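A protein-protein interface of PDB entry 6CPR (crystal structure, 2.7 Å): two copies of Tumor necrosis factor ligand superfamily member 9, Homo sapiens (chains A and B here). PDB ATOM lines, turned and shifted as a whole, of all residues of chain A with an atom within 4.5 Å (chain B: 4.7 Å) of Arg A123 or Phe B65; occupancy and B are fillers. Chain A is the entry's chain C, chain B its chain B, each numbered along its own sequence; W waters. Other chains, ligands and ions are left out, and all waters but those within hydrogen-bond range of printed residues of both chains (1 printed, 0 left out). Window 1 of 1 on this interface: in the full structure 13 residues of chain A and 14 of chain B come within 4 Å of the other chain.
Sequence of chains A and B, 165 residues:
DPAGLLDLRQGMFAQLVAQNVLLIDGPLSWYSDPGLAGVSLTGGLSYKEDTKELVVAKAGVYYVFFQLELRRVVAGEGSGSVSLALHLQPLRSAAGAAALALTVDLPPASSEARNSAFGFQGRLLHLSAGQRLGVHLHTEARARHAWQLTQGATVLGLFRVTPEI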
ATOM      1  N   TYR A  62      -8.925   3.081  10.481  1.00  0.00           N
ATOM      2  CA  TYR A  62      -9.330   4.461  10.596  1.00  0.00           C
ATOM      3  C   TYR A  62      -8.219   5.328  10.046  1.00  0.00           C
ATOM      4  O   TYR A  62      -7.056   4.994  10.182  1.00  0.00           O
ATOM      5  CB  TYR A  62      -9.565   4.809  12.056  1.00  0.00           C
ATOM      6  CG  TYR A  62     -10.788   4.172  12.675  1.00  0.00           C
ATOM      7  CD1 TYR A  62     -10.769   2.852  13.108  1.00  0.00           C
ATOM      8  CD2 TYR A  62     -11.958   4.898  12.858  1.00  0.00           C
ATOM      9  CE1 TYR A  62     -11.893   2.267  13.687  1.00  0.00           C
ATOM     10  CE2 TYR A  62     -13.082   4.331  13.444  1.00  0.00           C
ATOM     11  CZ  TYR A  62     -13.047   3.015  13.858  1.00  0.00           C
ATOM     12  OH  TYR A  62     -14.170   2.460  14.440  1.00  0.00           O
ATOM     13  N   TYR A  63      -8.605   6.419   9.395  1.00  0.00           N
ATOM     14  CA  TYR A  63      -7.725   7.562   9.226  1.00  0.00           C
ATOM     15  C   TYR A  63      -7.779   8.379  10.551  1.00  0.00           C
ATOM     16  O   TYR A  63      -8.846   8.829  10.976  1.00  0.00           O
ATOM     17  CB  TYR A  63      -8.155   8.397   8.011  1.00  0.00           C
ATOM     18  CG  TYR A  63      -7.273   9.601   7.694  1.00  0.00           C
ATOM     19  CD1 TYR A  63      -6.005   9.448   7.164  1.00  0.00           C
ATOM     20  CD2 TYR A  63      -7.729  10.888   7.900  1.00  0.00           C
ATOM     21  CE1 TYR A  63      -5.216  10.548   6.860  1.00  0.00           C
ATOM     22  CE2 TYR A  63      -6.952  11.984   7.603  1.00  0.00           C
ATOM     23  CZ  TYR A  63      -5.693  11.815   7.087  1.00  0.00           C
ATOM     24  OH  TYR A  63      -4.938  12.941   6.794  1.00  0.00           O
ATOM     25  N   VAL A  64      -6.634   8.518  11.201  1.00  0.00           N
ATOM     26  CA  VAL A  64      -6.535   9.279  12.426  1.00  0.00           C
ATOM     27  C   VAL A  64      -5.604  10.471  12.191  1.00  0.00           C
ATOM     28  O   VAL A  64      -4.519  10.333  11.631  1.00  0.00           O
ATOM     29  CB  VAL A  64      -6.008   8.407  13.568  1.00  0.00           C
ATOM     30  CG1 VAL A  64      -6.028   9.161  14.891  1.00  0.00           C
ATOM     31  CG2 VAL A  64      -6.847   7.140  13.680  1.00  0.00           C
ATOM     32  N   ALA A  99       1.654   5.475  18.166  1.00  0.00           N
ATOM     33  CA  ALA A  99       0.955   5.222  16.889  1.00  0.00           C
ATOM     34  C   ALA A  99       0.987   6.401  15.900  1.00  0.00           C
ATOM     35  O   ALA A  99       0.952   6.208  14.674  1.00  0.00           O
ATOM     36  CB  ALA A  99      -0.487   4.834  17.172  1.00  0.00           C
ATOM     37  N   LEU A 100       1.044   7.610  16.456  1.00  0.00           N
ATOM     38  CA  LEU A 100       1.071   8.847  15.704  1.00  0.00           C
ATOM     39  C   LEU A 100       1.869   9.879  16.541  1.00  0.00           C
ATOM     40  O   LEU A 100       1.714   9.947  17.768  1.00  0.00           O
ATOM     41  CB  LEU A 100      -0.379   9.285  15.484  1.00  0.00           C
ATOM     42  CG  LEU A 100      -0.673  10.376  14.455  1.00  0.00           C
ATOM     43  CD1 LEU A 100      -0.439   9.876  13.039  1.00  0.00           C
ATOM     44  CD2 LEU A 100      -2.106  10.878  14.614  1.00  0.00           C
ATOM     45  N   GLY A 122      -1.361  12.911   9.818  1.00  0.00           N
ATOM     46  CA  GLY A 122      -2.421  11.927   9.615  1.00  0.00           C
ATOM     47  C   GLY A 122      -1.858  10.616   9.115  1.00  0.00           C
ATOM     48  O   GLY A 122      -0.869  10.612   8.376  1.00  0.00           O
ATOM     49  N   ARG A 123      -2.446   9.507   9.569  1.00  0.00           N
ATOM     50  CA  ARG A 123      -2.279   8.216   8.904  1.00  0.00           C
ATOM     51  C   ARG A 123      -3.437   7.224   9.154  1.00  0.00           C
ATOM     52  O   ARG A 123      -4.326   7.451   9.983  1.00  0.00           O
ATOM     53  CB  ARG A 123      -0.934   7.582   9.275  1.00  0.00           C
ATOM     54  CG  ARG A 123      -0.848   7.045  10.690  1.00  0.00           C
ATOM     55  CD  ARG A 123       0.600   6.970  11.188  1.00  0.00           C
ATOM     56  NE  ARG A 123       1.264   5.693  10.917  1.00  0.00           N
ATOM     57  CZ  ARG A 123       2.585   5.510  10.854  1.00  0.00           C
ATOM     58  NH1 ARG A 123       3.435   6.531  11.018  1.00  0.00           N
ATOM     59  NH2 ARG A 123       3.072   4.288  10.611  1.00  0.00           N
ATOM     60  N   LEU A 124      -3.396   6.119   8.413  1.00  0.00           N
ATOM     61  CA  LEU A 124      -4.296   4.986   8.619  1.00  0.00           C
ATOM     62  C   LEU A 124      -3.773   4.105   9.761  1.00  0.00           C
ATOM     63  O   LEU A 124      -2.613   3.715   9.754  1.00  0.00           O
ATOM     64  CB  LEU A 124      -4.435   4.171   7.334  1.00  0.00           C
ATOM     65  CG  LEU A 124      -5.004   4.949   6.148  1.00  0.00           C
ATOM     66  CD1 LEU A 124      -4.778   4.215   4.840  1.00  0.00           C
ATOM     67  CD2 LEU A 124      -6.485   5.238   6.326  1.00  0.00           C
ATOM     68  N   LEU A 125      -4.626   3.832  10.748  1.00  0.00           N
ATOM     69  CA  LEU A 125      -4.305   2.963  11.896  1.00  0.00           C
ATOM     70  C   LEU A 125      -5.324   1.861  11.992  1.00  0.00           C
ATOM     71  O   LEU A 125      -6.515   2.099  11.840  1.00  0.00           O
ATOM     72  CB  LEU A 125      -4.376   3.728  13.220  1.00  0.00           C
ATOM     73  CG  LEU A 125      -3.388   4.852  13.498  1.00  0.00           C
ATOM     74  CD1 LEU A 125      -3.605   5.340  14.923  1.00  0.00           C
ATOM     75  CD2 LEU A 125      -1.945   4.420  13.308  1.00  0.00           C
ATOM     76  N   GLN B  15      -1.407   1.498   2.913  1.00  0.00           N
ATOM     77  CA  GLN B  15      -0.394   2.300   3.533  1.00  0.00           C
ATOM     78  C   GLN B  15       0.911   1.553   3.459  1.00  0.00           C
ATOM     79  O   GLN B  15       0.954   0.371   3.694  1.00  0.00           O
ATOM     80  CB  GLN B  15      -0.750   2.571   4.974  1.00  0.00           C
ATOM     81  CG  GLN B  15       0.102   3.655   5.578  1.00  0.00           C
ATOM     82  CD  GLN B  15      -0.416   4.110   6.913  1.00  0.00           C
ATOM     83  OE1 GLN B  15      -1.133   5.096   7.011  1.00  0.00           O
ATOM     84  NE2 GLN B  15      -0.062   3.386   7.954  1.00  0.00           N
ATOM     85  N   GLY B  38       2.019  -0.531  10.838  1.00  0.00           N
ATOM     86  CA  GLY B  38       1.920   0.669  10.015  1.00  0.00           C
ATOM     87  C   GLY B  38       1.735   0.397   8.538  1.00  0.00           C
ATOM     88  O   GLY B  38       1.642   1.334   7.754  1.00  0.00           O
ATOM     89  N   TYR B  63      -8.126   9.765  -1.840  1.00  0.00           N
ATOM     90  CA  TYR B  63      -7.323  10.659  -1.025  1.00  0.00           C
ATOM     91  C   TYR B  63      -5.958   9.979  -0.868  1.00  0.00           C
ATOM     92  O   TYR B  63      -5.876   8.868  -0.369  1.00  0.00           O
ATOM     93  CB  TYR B  63      -8.001  10.919   0.320  1.00  0.00           C
ATOM     94  CG  TYR B  63      -7.265  11.869   1.257  1.00  0.00           C
ATOM     95  CD1 TYR B  63      -7.220  13.231   1.013  1.00  0.00           C
ATOM     96  CD2 TYR B  63      -6.655  11.394   2.410  1.00  0.00           C
ATOM     97  CE1 TYR B  63      -6.572  14.093   1.889  1.00  0.00           C
ATOM     98  CE2 TYR B  63      -6.017  12.238   3.284  1.00  0.00           C
ATOM     99  CZ  TYR B  63      -5.978  13.592   3.023  1.00  0.00           C
ATOM    100  OH  TYR B  63      -5.334  14.401   3.918  1.00  0.00           O
ATOM    101  N   VAL B  64      -4.908  10.644  -1.334  1.00  0.00           N
ATOM    102  CA  VAL B  64      -3.551  10.131  -1.249  1.00  0.00           C
ATOM    103  C   VAL B  64      -2.754  11.105  -0.392  1.00  0.00           C
ATOM    104  O   VAL B  64      -2.828  12.313  -0.582  1.00  0.00           O
ATOM    105  CB  VAL B  64      -2.911  10.001  -2.644  1.00  0.00           C
ATOM    106  CG1 VAL B  64      -1.535   9.351  -2.575  1.00  0.00           C
ATOM    107  CG2 VAL B  64      -3.823   9.195  -3.572  1.00  0.00           C
ATOM    108  N   PHE B  65      -2.014  10.572   0.568  1.00  0.00           N
ATOM    109  CA  PHE B  65      -1.181  11.379   1.431  1.00  0.00           C
ATOM    110  C   PHE B  65       0.193  10.732   1.606  1.00  0.00           C
ATOM    111  O   PHE B  65       0.335   9.506   1.515  1.00  0.00           O
ATOM    112  CB  PHE B  65      -1.842  11.585   2.792  1.00  0.00           C
ATOM    113  CG  PHE B  65      -2.137  10.303   3.527  1.00  0.00           C
ATOM    114  CD1 PHE B  65      -1.226   9.780   4.433  1.00  0.00           C
ATOM    115  CD2 PHE B  65      -3.337   9.603   3.297  1.00  0.00           C
ATOM    116  CE1 PHE B  65      -1.504   8.580   5.094  1.00  0.00           C
ATOM    117  CE2 PHE B  65      -3.605   8.410   3.954  1.00  0.00           C
ATOM    118  CZ  PHE B  65      -2.689   7.892   4.851  1.00  0.00           C
ATOM    119  N   PHE B  66       1.203  11.573   1.837  1.00  0.00           N
ATOM    120  CA  PHE B  66       2.466  11.080   2.343  1.00  0.00           C
ATOM    121  C   PHE B  66       3.059  11.942   3.427  1.00  0.00           C
ATOM    122  O   PHE B  66       2.800  13.128   3.513  1.00  0.00           O
ATOM    123  CB  PHE B  66       3.512  10.687   1.273  1.00  0.00           C
ATOM    124  CG  PHE B  66       3.803  11.711   0.207  1.00  0.00           C
ATOM    125  CD1 PHE B  66       3.488  13.062   0.321  1.00  0.00           C
ATOM    126  CD2 PHE B  66       4.479  11.292  -0.922  1.00  0.00           C
ATOM    127  CE1 PHE B  66       3.802  13.954  -0.696  1.00  0.00           C
ATOM    128  CE2 PHE B  66       4.797  12.176  -1.938  1.00  0.00           C
ATOM    129  CZ  PHE B  66       4.460  13.511  -1.826  1.00  0.00           C
ATOM    130  N   GLN B  67       3.815  11.262   4.277  1.00  0.00           N
ATOM    131  CA  GLN B  67       4.356  11.773   5.501  1.00  0.00           C
ATOM    132  C   GLN B  67       5.860  11.662   5.295  1.00  0.00           C
ATOM    133  O   GLN B  67       6.340  10.742   4.632  1.00  0.00           O
ATOM    134  CB  GLN B  67       3.885  10.878   6.637  1.00  0.00           C
ATOM    135  CG  GLN B  67       3.881  11.499   8.021  1.00  0.00           C
ATOM    136  CD  GLN B  67       3.257  10.566   9.061  1.00  0.00           C
ATOM    137  OE1 GLN B  67       2.125  10.094   8.903  1.00  0.00           O
ATOM    138  NE2 GLN B  67       3.998  10.293  10.129  1.00  0.00           N
ATOM    139  N   LEU B 100       1.776  14.729  -6.449  1.00  0.00           N
ATOM    140  CA  LEU B 100       1.834  15.148  -5.062  1.00  0.00           C
ATOM    141  C   LEU B 100       3.307  15.432  -4.756  1.00  0.00           C
ATOM    142  O   LEU B 100       4.172  14.670  -5.194  1.00  0.00           O
ATOM    143  CB  LEU B 100       1.297  14.004  -4.206  1.00  0.00           C
ATOM    144  CG  LEU B 100       0.949  14.277  -2.751  1.00  0.00           C
ATOM    145  CD1 LEU B 100      -0.280  15.160  -2.638  1.00  0.00           C
ATOM    146  CD2 LEU B 100       0.722  12.960  -2.015  1.00  0.00           C
ATOM    147  N   PHE B 120       3.809  16.776   6.050  1.00  0.00           N
ATOM    148  CA  PHE B 120       2.626  16.045   5.639  1.00  0.00           C
ATOM    149  C   PHE B 120       1.956  16.799   4.489  1.00  0.00           C
ATOM    150  O   PHE B 120       1.856  18.025   4.521  1.00  0.00           O
ATOM    151  CB  PHE B 120       1.650  15.904   6.796  1.00  0.00           C
ATOM    152  CG  PHE B 120       0.433  15.147   6.442  1.00  0.00           C
ATOM    153  CD1 PHE B 120       0.390  13.796   6.624  1.00  0.00           C
ATOM    154  CD2 PHE B 120      -0.652  15.774   5.886  1.00  0.00           C
ATOM    155  CE1 PHE B 120      -0.722  13.073   6.281  1.00  0.00           C
ATOM    156  CE2 PHE B 120      -1.772  15.049   5.536  1.00  0.00           C
ATOM    157  CZ  PHE B 120      -1.804  13.699   5.742  1.00  0.00           C
ATOM    158  N   GLN B 121       1.524  16.051   3.477  1.00  0.00           N
ATOM    159  CA  GLN B 121       0.679  16.569   2.425  1.00  0.00           C
ATOM    160  C   GLN B 121      -0.341  15.519   1.975  1.00  0.00           C
ATOM    161  O   GLN B 121      -0.045  14.328   1.920  1.00  0.00           O
ATOM    162  CB  GLN B 121       1.523  17.007   1.247  1.00  0.00           C
ATOM    163  CG  GLN B 121       0.741  17.769   0.198  1.00  0.00           C
ATOM    164  CD  GLN B 121       1.642  18.276  -0.901  1.00  0.00           C
ATOM    165  OE1 GLN B 121       1.540  17.840  -2.044  1.00  0.00           O
ATOM    166  NE2 GLN B 121       2.545  19.198  -0.555  1.00  0.00           N
ATOM    167  N   GLY B 122      -1.531  15.996   1.628  1.00  0.00           N
ATOM    168  CA  GLY B 122      -2.601  15.163   1.144  1.00  0.00           C
ATOM    169  C   GLY B 122      -3.393  15.887   0.082  1.00  0.00           C
ATOM    170  O   GLY B 122      -3.504  17.106   0.139  1.00  0.00           O
ATOM    171  N   GLY B 152       9.956   4.071  10.127  1.00  0.00           N
ATOM    172  CA  GLY B 152       8.557   3.874  10.462  1.00  0.00           C
ATOM    173  C   GLY B 152       7.728   5.147  10.450  1.00  0.00           C
ATOM    174  O   GLY B 152       6.665   5.192  11.088  1.00  0.00           O
ATOM    175  N   ALA B 153       8.209   6.180   9.750  1.00  0.00           N
ATOM    176  CA  ALA B 153       7.563   7.512   9.752  1.00  0.00           C
ATOM    177  C   ALA B 153       7.407   8.189   8.376  1.00  0.00           C
ATOM    178  O   ALA B 153       6.661   9.163   8.252  1.00  0.00           O
ATOM    179  CB  ALA B 153       8.302   8.438  10.708  1.00  0.00           C
ATOM    180  N   VAL B 155       5.757   7.597   5.181  1.00  0.00           N
ATOM    181  CA  VAL B 155       4.604   6.770   4.886  1.00  0.00           C
ATOM    182  C   VAL B 155       3.936   7.309   3.620  1.00  0.00           C
ATOM    183  O   VAL B 155       3.841   8.523   3.431  1.00  0.00           O
ATOM    184  CB  VAL B 155       3.612   6.817   6.071  1.00  0.00           C
ATOM    185  CG1 VAL B 155       2.337   6.053   5.791  1.00  0.00           C
ATOM    186  CG2 VAL B 155       4.260   6.261   7.320  1.00  0.00           C
ATOM    187  N   LEU B 156       3.517   6.395   2.750  1.00  0.00           N
ATOM    188  CA  LEU B 156       2.608   6.720   1.656  1.00  0.00           C
ATOM    189  C   LEU B 156       1.292   6.007   1.931  1.00  0.00           C
ATOM    190  O   LEU B 156       1.297   4.829   2.228  1.00  0.00           O
ATOM    191  CB  LEU B 156       3.175   6.277   0.301  1.00  0.00           C
ATOM    192  CG  LEU B 156       2.236   6.352  -0.920  1.00  0.00           C
ATOM    193  CD1 LEU B 156       1.969   7.811  -1.293  1.00  0.00           C
ATOM    194  CD2 LEU B 156       2.801   5.556  -2.101  1.00  0.00           C
ATOM    195  N   GLY B 157       0.180   6.722   1.820  1.00  0.00           N
ATOM    196  CA  GLY B 157      -1.124   6.133   2.031  1.00  0.00           C
ATOM    197  C   GLY B 157      -2.189   6.600   1.067  1.00  0.00           C
ATOM    198  O   GLY B 157      -2.068   7.636   0.421  1.00  0.00           O
ATOM    199  N   LEU B 158      -3.242   5.803   0.980  1.00  0.00           N
ATOM    200  CA  LEU B 158      -4.417   6.172   0.225  1.00  0.00           C
ATOM    201  C   LEU B 158      -5.603   5.307   0.581  1.00  0.00           C
ATOM    202  O   LEU B 158      -5.464   4.148   0.984  1.00  0.00           O
ATOM    203  CB  LEU B 158      -4.168   6.062  -1.278  1.00  0.00           C
ATOM    204  CG  LEU B 158      -3.663   4.719  -1.795  1.00  0.00           C
ATOM    205  CD1 LEU B 158      -4.787   3.858  -2.312  1.00  0.00           C
ATOM    206  CD2 LEU B 158      -2.704   4.932  -2.933  1.00  0.00           C
ATOM    207  N   PHE B 159      -6.776   5.890   0.420  1.00  0.00           N
ATOM    208  CA  PHE B 159      -8.013   5.159   0.490  1.00  0.00           C
ATOM    209  C   PHE B 159      -8.964   5.714  -0.556  1.00  0.00           C
ATOM    210  O   PHE B 159      -8.848   6.876  -0.978  1.00  0.00           O
ATOM    211  CB  PHE B 159      -8.615   5.186   1.907  1.00  0.00           C
ATOM    212  CG  PHE B 159      -8.854   6.570   2.461  1.00  0.00           C
ATOM    213  CD1 PHE B 159     -10.082   7.200   2.288  1.00  0.00           C
ATOM    214  CD2 PHE B 159      -7.850   7.240   3.175  1.00  0.00           C
ATOM    215  CE1 PHE B 159     -10.312   8.465   2.808  1.00  0.00           C
ATOM    216  CE2 PHE B 159      -8.080   8.507   3.693  1.00  0.00           C
ATOM    217  CZ  PHE B 159      -9.312   9.119   3.507  1.00  0.00           C
HETATM  218  O   HOH W   1       5.371   6.323  13.912  1.00  0.00           O
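The backbone NH of Leu A124 sits at hydrogen-bond distance from the side-chain amide oxygen of Gln B15 (2.9 Å).
The side-chain hydroxyl of Tyr B63 lies within hydrogen-bond range of the side-chain hydroxyl of Tyr A63, at 3.2 Å.
The side-chain amide oxygen (OE1) of Gln B67 sits close to the backbone carbonyl oxygen (O) of Gly A122 (3.1 Å).
The guanidinium group (NH1) of Arg A123 lies within hydrogen-bond range of the backbone carbonyl oxygen (O) of Gly B152, 3.5 Å away.
The side-chain amide nitrogen of Gln B15 sits at hydrogen-bond distance from the backbone carbonyl oxygen of Gly B38, 2.7 Å away.
O of Phe B159 lies within hydrogen-bond range of N of Tyr B63, 3.1 Å away.
The backbone NH of Gly B157 is in hydrogen-bond range of the backbone carbonyl oxygen of Phe B65.
The side-chain amide nitrogen (NE2) of Gln B67 sits at hydrogen-bond distance from the backbone carbonyl oxygen (O) of Ala B153 (3.4 Å).
N of Gln B67 is in hydrogen-bond range of O of Val B155, at 2.9 Å.
The backbone carbonyl oxygen of Arg A123 is in hydrogen-bond range of the backbone NH of Val A64.
Tyr A63 touches Phe B65 (CE1 to CE2, 3.95 Å).
CZ of Phe B120 touches OH of Tyr A63, 3.4 Å away.
O of Gly A122 touches CE1 of Phe B65 (3.9 Å).
Gly A122 touches Phe B120 (O to CE1, 3.2 Å).
OE1 of Gln B15 touches CB of Arg A123 (3.4 Å).
NE2 of Gln B67 touches NH1 of Arg A123, at 3.9 Å.
Arg A123 touches Val B155.
CG of Leu A124 touches CZ of Phe B65, at 3.96 Å.
O of Leu B158 touches CD1 of Leu A124, 3.9 Å away.
Leu A124 touches Phe B159.
Arg A123 touches just these residues of chain B: Gln B15 (3.4 Å), Gly B38 (3.8 Å), Phe B65 (3.9 Å), Gln B67 (3.9 Å), Gly B152 (3.5 Å) and Val B155 (3.8 Å).
Phe B65 touches four residues of chain A.
Of the printed residues of chain A, Gly B152 touches Arg A123.
Printed residues of chain A within 4 Å of Tyr B63: Tyr A63.
Of the printed residues of chain A, Val B155 touches Arg A123 (3.8 Å).
Ala B153 touches none of the printed residues of chain A.
The nearest printed residue of chain A that does not touch Phe B65 is Val A64 (7.4 Å).
The nearest printed residue of chain A that does not touch Gly B38 is Leu A124 (5.3 Å).
Of the 18 printed residues of chain B, 10 touch a printed residue of chain A.
Hydrophobic or aromatic side chains of chain B that line the printed part of chain A: Tyr B63, Phe B65, Phe B120, Val B155 and Phe B159.
Along chain B the printed residues that touch a printed residue of chain A span positions 15 to 159.
Among the printed residues, 16 pairs touch across the chains.
Among the printed residues, no Asp or Glu carboxylate lies within 4 Å of a Lys or Arg side-chain nitrogen of the other chain.
Tyr A63 touches its own counterpart, Tyr B63.
4 positions are printed for both chains.
Water W1 lies within hydrogen-bond range of O of Gly B152 (3.3 Å) and NH1 of Arg A123 (3.5 Å).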
